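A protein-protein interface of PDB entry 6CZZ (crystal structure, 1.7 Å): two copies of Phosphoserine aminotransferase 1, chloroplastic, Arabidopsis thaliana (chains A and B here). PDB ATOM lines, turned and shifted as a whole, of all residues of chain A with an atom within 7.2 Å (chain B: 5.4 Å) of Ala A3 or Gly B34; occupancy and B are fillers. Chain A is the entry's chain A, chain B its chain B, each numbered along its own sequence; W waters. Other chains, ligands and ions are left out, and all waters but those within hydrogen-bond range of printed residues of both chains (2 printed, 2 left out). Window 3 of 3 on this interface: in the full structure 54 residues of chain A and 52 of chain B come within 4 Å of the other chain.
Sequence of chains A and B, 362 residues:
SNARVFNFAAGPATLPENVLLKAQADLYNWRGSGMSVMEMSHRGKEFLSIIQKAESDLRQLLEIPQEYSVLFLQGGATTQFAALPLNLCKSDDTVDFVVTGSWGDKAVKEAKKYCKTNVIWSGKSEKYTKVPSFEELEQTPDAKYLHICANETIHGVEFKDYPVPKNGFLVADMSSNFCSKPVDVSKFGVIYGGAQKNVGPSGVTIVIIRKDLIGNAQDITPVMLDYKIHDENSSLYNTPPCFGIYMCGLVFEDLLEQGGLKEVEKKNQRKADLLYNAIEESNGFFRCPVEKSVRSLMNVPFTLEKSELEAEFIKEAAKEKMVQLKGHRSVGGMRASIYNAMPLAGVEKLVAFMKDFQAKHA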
ATOM      1  N   ALA A   3      17.690   8.802   8.719  1.00  0.00           N
ATOM      2  CA  ALA A   3      16.782   8.637   9.861  1.00  0.00           C
ATOM      3  C   ALA A   3      15.508   7.914   9.442  1.00  0.00           C
ATOM      4  O   ALA A   3      15.131   7.954   8.287  1.00  0.00           O
ATOM      5  CB  ALA A   3      16.437   9.982  10.479  1.00  0.00           C
ATOM      6  N   ARG A   4      14.840   7.260  10.388  1.00  0.00           N
ATOM      7  CA  ARG A   4      13.535   6.699  10.077  1.00  0.00           C
ATOM      8  C   ARG A   4      12.582   7.827   9.714  1.00  0.00           C
ATOM      9  O   ARG A   4      12.695   8.945  10.212  1.00  0.00           O
ATOM     10  CB  ARG A   4      12.997   5.869  11.246  1.00  0.00           C
ATOM     11  CG  ARG A   4      13.560   4.432  11.158  1.00  0.00           C
ATOM     12  CD  ARG A   4      13.184   3.589  12.304  1.00  0.00           C
ATOM     13  NE  ARG A   4      11.759   3.407  12.476  1.00  0.00           N
ATOM     14  CZ  ARG A   4      11.072   2.437  11.896  1.00  0.00           C
ATOM     15  NH1 ARG A   4      11.694   1.558  11.106  1.00  0.00           N
ATOM     16  NH2 ARG A   4       9.777   2.318  12.146  1.00  0.00           N
ATOM     17  N   VAL A   5      11.671   7.536   8.803  1.00  0.00           N
ATOM     18  CA  VAL A   5      10.709   8.507   8.337  1.00  0.00           C
ATOM     19  C   VAL A   5       9.383   8.271   9.048  1.00  0.00           C
ATOM     20  O   VAL A   5       9.176   7.250   9.704  1.00  0.00           O
ATOM     21  CB  VAL A   5      10.551   8.431   6.810  1.00  0.00           C
ATOM     22  CG1 VAL A   5      11.833   8.822   6.164  1.00  0.00           C
ATOM     23  CG2 VAL A   5      10.191   7.030   6.430  1.00  0.00           C
ATOM     24  N   PHE A   6       8.463   9.231   8.920  1.00  0.00           N
ATOM     25  CA  PHE A   6       7.070   8.953   9.250  1.00  0.00           C
ATOM     26  C   PHE A   6       6.423   8.314   8.034  1.00  0.00           C
ATOM     27  O   PHE A   6       6.410   8.895   6.947  1.00  0.00           O
ATOM     28  CB  PHE A   6       6.365  10.241   9.668  1.00  0.00           C
ATOM     29  CG  PHE A   6       6.898  10.800  10.960  1.00  0.00           C
ATOM     30  CD1 PHE A   6       6.854  10.042  12.113  1.00  0.00           C
ATOM     31  CD2 PHE A   6       7.408  12.062  11.021  1.00  0.00           C
ATOM     32  CE1 PHE A   6       7.308  10.545  13.317  1.00  0.00           C
ATOM     33  CE2 PHE A   6       7.903  12.576  12.224  1.00  0.00           C
ATOM     34  CZ  PHE A   6       7.848  11.785  13.374  1.00  0.00           C
ATOM     35  N   ASN A   7       5.979   7.101   8.193  1.00  0.00           N
ATOM     36  CA  ASN A   7       5.597   6.252   7.079  1.00  0.00           C
ATOM     37  C   ASN A   7       4.084   6.076   7.108  1.00  0.00           C
ATOM     38  O   ASN A   7       3.550   5.323   7.940  1.00  0.00           O
ATOM     39  CB  ASN A   7       6.345   4.920   7.186  1.00  0.00           C
ATOM     40  CG  ASN A   7       5.805   3.868   6.271  1.00  0.00           C
ATOM     41  OD1 ASN A   7       5.105   4.158   5.292  1.00  0.00           O
ATOM     42  ND2 ASN A   7       6.107   2.597   6.613  1.00  0.00           N
ATOM     43  N   GLU A  17       8.746   0.791  17.039  1.00  0.00           N
ATOM     44  CA  GLU A  17      10.209   0.705  17.015  1.00  0.00           C
ATOM     45  C   GLU A  17      10.733  -0.269  18.058  1.00  0.00           C
ATOM     46  O   GLU A  17      11.706  -1.000  17.789  1.00  0.00           O
ATOM     47  CB  GLU A  17      10.818   2.093  17.181  1.00  0.00           C
ATOM     48  CG  GLU A  17      10.546   2.935  15.894  1.00  0.00           C
ATOM     49  CD  GLU A  17      11.217   4.302  15.869  1.00  0.00           C
ATOM     50  OE1 GLU A  17      11.673   4.745  16.937  1.00  0.00           O
ATOM     51  OE2 GLU A  17      11.277   4.927  14.776  1.00  0.00           O
ATOM     52  N   LYS A 321      10.504  13.957   5.320  1.00  0.00           N
ATOM     53  CA  LYS A 321      10.470  12.651   5.999  1.00  0.00           C
ATOM     54  C   LYS A 321       9.054  12.209   6.360  1.00  0.00           C
ATOM     55  O   LYS A 321       8.846  11.517   7.362  1.00  0.00           O
ATOM     56  CB  LYS A 321      11.362  12.634   7.246  1.00  0.00           C
ATOM     57  CG  LYS A 321      12.777  13.138   6.999  1.00  0.00           C
ATOM     58  CD  LYS A 321      13.826  12.235   7.659  1.00  0.00           C
ATOM     59  CE  LYS A 321      15.239  12.646   7.245  1.00  0.00           C
ATOM     60  NZ  LYS A 321      16.249  11.555   7.496  1.00  0.00           N
ATOM     61  N   VAL A 323       6.379  10.068   4.268  1.00  0.00           N
ATOM     62  CA  VAL A 323       6.339   9.363   2.988  1.00  0.00           C
ATOM     63  C   VAL A 323       5.041   8.579   2.866  1.00  0.00           C
ATOM     64  O   VAL A 323       4.330   8.350   3.840  1.00  0.00           O
ATOM     65  CB  VAL A 323       7.543   8.434   2.781  1.00  0.00           C
ATOM     66  CG1 VAL A 323       8.824   9.220   2.904  1.00  0.00           C
ATOM     67  CG2 VAL A 323       7.527   7.293   3.805  1.00  0.00           C
ATOM     68  N   TYR B  28      15.948  -2.634  11.106  1.00  0.00           N
ATOM     69  CA  TYR B  28      15.351  -1.390  11.560  1.00  0.00           C
ATOM     70  C   TYR B  28      15.277  -0.339  10.459  1.00  0.00           C
ATOM     71  O   TYR B  28      14.358   0.505  10.455  1.00  0.00           O
ATOM     72  CB  TYR B  28      16.177  -0.839  12.725  1.00  0.00           C
ATOM     73  CG  TYR B  28      15.597   0.321  13.516  1.00  0.00           C
ATOM     74  CD1 TYR B  28      14.450   0.155  14.291  1.00  0.00           C
ATOM     75  CD2 TYR B  28      16.235   1.545  13.552  1.00  0.00           C
ATOM     76  CE1 TYR B  28      13.920   1.209  15.059  1.00  0.00           C
ATOM     77  CE2 TYR B  28      15.705   2.606  14.312  1.00  0.00           C
ATOM     78  CZ  TYR B  28      14.533   2.394  15.069  1.00  0.00           C
ATOM     79  OH  TYR B  28      13.971   3.391  15.862  1.00  0.00           O
ATOM     80  N   ASN B  29      16.236  -0.357   9.526  1.00  0.00           N
ATOM     81  CA  ASN B  29      16.333   0.709   8.528  1.00  0.00           C
ATOM     82  C   ASN B  29      17.064   0.111   7.322  1.00  0.00           C
ATOM     83  O   ASN B  29      18.293   0.024   7.325  1.00  0.00           O
ATOM     84  CB  ASN B  29      17.065   1.924   9.073  1.00  0.00           C
ATOM     85  CG  ASN B  29      17.028   3.107   8.096  1.00  0.00           C
ATOM     86  OD1 ASN B  29      16.806   2.918   6.903  1.00  0.00           O
ATOM     87  ND2 ASN B  29      17.245   4.314   8.594  1.00  0.00           N
ATOM     88  N   TRP B  30      16.316  -0.315   6.333  1.00  0.00           N
ATOM     89  CA  TRP B  30      16.923  -0.960   5.166  1.00  0.00           C
ATOM     90  C   TRP B  30      17.516   0.085   4.218  1.00  0.00           C
ATOM     91  O   TRP B  30      16.791   0.912   3.656  1.00  0.00           O
ATOM     92  CB  TRP B  30      15.889  -1.823   4.455  1.00  0.00           C
ATOM     93  CG  TRP B  30      16.421  -2.592   3.254  1.00  0.00           C
ATOM     94  CD1 TRP B  30      16.967  -3.873   3.252  1.00  0.00           C
ATOM     95  CD2 TRP B  30      16.382  -2.180   1.890  1.00  0.00           C
ATOM     96  NE1 TRP B  30      17.304  -4.230   1.968  1.00  0.00           N
ATOM     97  CE2 TRP B  30      16.938  -3.223   1.116  1.00  0.00           C
ATOM     98  CE3 TRP B  30      15.915  -1.030   1.239  1.00  0.00           C
ATOM     99  CZ2 TRP B  30      17.056  -3.142  -0.265  1.00  0.00           C
ATOM    100  CZ3 TRP B  30      16.028  -0.951  -0.145  1.00  0.00           C
ATOM    101  CH2 TRP B  30      16.599  -1.993  -0.875  1.00  0.00           C
ATOM    102  N   GLY B  32      19.086   2.905   4.347  1.00  0.00           N
ATOM    103  CA  GLY B  32      18.767   4.303   4.531  1.00  0.00           C
ATOM    104  C   GLY B  32      17.430   4.730   3.981  1.00  0.00           C
ATOM    105  O   GLY B  32      17.206   5.933   3.790  1.00  0.00           O
ATOM    106  N   SER B  33      16.529   3.785   3.719  1.00  0.00           N
ATOM    107  CA  SER B  33      15.156   4.100   3.350  1.00  0.00           C
ATOM    108  C   SER B  33      14.352   4.650   4.521  1.00  0.00           C
ATOM    109  O   SER B  33      13.226   5.110   4.323  1.00  0.00           O
ATOM    110  CB  SER B  33      14.453   2.857   2.804  1.00  0.00           C
ATOM    111  OG  SER B  33      14.199   1.894   3.836  1.00  0.00           O
ATOM    112  N   GLY B  34      14.876   4.566   5.734  1.00  0.00           N
ATOM    113  CA  GLY B  34      14.150   5.002   6.890  1.00  0.00           C
ATOM    114  C   GLY B  34      13.059   4.062   7.342  1.00  0.00           C
ATOM    115  O   GLY B  34      12.224   4.473   8.141  1.00  0.00           O
ATOM    116  N   MET B  35      13.034   2.819   6.864  1.00  0.00           N
ATOM    117  CA  MET B  35      12.050   1.880   7.389  1.00  0.00           C
ATOM    118  C   MET B  35      12.567   0.464   7.222  1.00  0.00           C
ATOM    119  O   MET B  35      13.510   0.218   6.472  1.00  0.00           O
ATOM    120  CB  MET B  35      10.711   2.065   6.677  1.00  0.00           C
ATOM    121  CG  MET B  35      10.723   1.577   5.263  1.00  0.00           C
ATOM    122  SD  MET B  35       9.195   2.057   4.380  1.00  0.00           S
ATOM    123  CE  MET B  35       9.213   3.757   4.600  1.00  0.00           C
ATOM    124  N   SER B  36      11.936  -0.476   7.933  1.00  0.00           N
ATOM    125  CA  SER B  36      12.222  -1.895   7.774  1.00  0.00           C
ATOM    126  C   SER B  36      11.611  -2.420   6.483  1.00  0.00           C
ATOM    127  O   SER B  36      10.589  -1.925   6.025  1.00  0.00           O
ATOM    128  CB  SER B  36      11.613  -2.661   8.961  1.00  0.00           C
ATOM    129  OG  SER B  36      11.799  -4.050   8.847  1.00  0.00           O
ATOM    130  N   GLU B  39       7.902  -2.902   6.840  1.00  0.00           N
ATOM    131  CA  GLU B  39       7.013  -1.740   6.818  1.00  0.00           C
ATOM    132  C   GLU B  39       6.874  -1.105   5.443  1.00  0.00           C
ATOM    133  O   GLU B  39       6.179  -0.089   5.300  1.00  0.00           O
ATOM    134  CB  GLU B  39       7.525  -0.658   7.770  1.00  0.00           C
ATOM    135  CG  GLU B  39       7.762  -1.160   9.168  1.00  0.00           C
ATOM    136  CD  GLU B  39       8.598  -0.175   9.950  1.00  0.00           C
ATOM    137  OE1 GLU B  39       9.781  -0.007   9.596  1.00  0.00           O
ATOM    138  OE2 GLU B  39       8.073   0.506  10.888  1.00  0.00           O
HETATM  139  O   HOH W   1       7.698   2.770   9.259  1.00  0.00           O
HETATM  140  O   HOH W   2       9.702   4.448   9.368  1.00  0.00           O
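No position is printed for both chains.
Of the 12 pairs that touch across the chains among the printed residues, none has its exchanged pair printed and touching as well.
Water W2 bridges O of Gly B34 (2.8 Å) and O of Val A5 (2.9 Å).
Water W1 bridges OE2 of Glu B39 (2.8 Å) and ND2 of Asn A7 (3.1 Å).
The guanidinium group (NE) of Arg A4 is in salt-bridge range of the side-chain carboxylate (OE2) of Glu A17 (2.8 Å).
The backbone carbonyl oxygen (O) of Phe A6 sits at hydrogen-bond distance from the backbone NH (N) of Val A323 (2.9 Å).
The side-chain amide oxygen of Asn B29 is in hydrogen-bond range of the backbone NH of Gly B34 (2.8 Å).
The backbone NH (N) of Trp B30 is in hydrogen-bond range of the backbone carbonyl oxygen (O) of Met B35 (2.9 Å).
The side-chain hydroxyl (OG) of Ser B33 lies within hydrogen-bond range of the backbone carbonyl oxygen (O) of Met B35 (3.2 Å).
The backbone NH (N) of Ser B36 lies within hydrogen-bond range of the side-chain carboxylate (OE1) of Glu B39.
Of chain B, only Gly B34 (3.4 Å) comes within 4 Å of Ala A3.
Gly B34 touches just these residues of chain A: Ala A3 (3.4 Å), Arg A4 (3.2 Å) and Val A5 (3.2 Å).
Printed residues of chain A within 4 Å of Tyr B28: Arg A4 (2.9 Å) and Glu A17 (2.9 Å).
Of the printed residues of chain B, Val A323 touches Met B35 (3.997 Å).
Of the printed residues of chain B, Val A5 touches Gly B34 and Met B35.
The nearest residue of chain B that does not touch Ala A3 is Asn B29 (4.1 Å).
The nearest residue of chain A that does not touch Gly B34 is Asn A7 (6.0 Å).
The nearest printed residue of chain B that does not touch Asn A7 is Gly B34 (6.0 Å).
Among the printed residues, pairs that only touch across the chains: Arg A4 with Gly B34 (3.2 Å), Ala A3 with Gly B34 (3.4 Å), Arg A4 with Met B35 (3.7 Å), Arg A4 with Ser B36 (3.8 Å), Asn A7 with Met B35 (3.8 Å), Val A5 with Met B35 (3.9 Å) and Val A323 with Met B35 (3.997 Å).
Printed residues of chain B that touch a printed residue of chain A: Tyr B28, Gly B34, Met B35, Ser B36 and Glu B39.
Hydrophobic or aromatic side chains of chain B that line the printed part of chain A: Tyr B28 and Met B35.
Along chain B the printed residues that touch a printed residue of chain A span positions 28 to 39.
Printed residues of chain A that touch a printed residue of chain B: Ala A3, Arg A4, Val A5, Asn A7, Glu A17 and Val A323.
Hydrophobic or aromatic side chains of chain A that line the printed part of chain B: Val A5 and Val A323.
Among the printed residues, 12 pairs touch across the chains.
NH1 of Arg A4 lies within hydrogen-bond range of O of Tyr B28, 2.9 Å away.
The side-chain carboxylate (OE2) of Glu B39 lies within salt-bridge range of the guanidinium group (NH2) of Arg A4 (2.8 Å).
The backbone NH of Val A5 sits at hydrogen-bond distance from the backbone carbonyl oxygen of Gly B34.
The backbone carbonyl oxygen of Glu B39 is in hydrogen-bond range of the side-chain amide nitrogen of Asn A7.
The side-chain carboxylate (OE1) of Glu A17 lies within hydrogen-bond range of the side-chain hydroxyl (OH) of Tyr B28 (2.9 Å).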
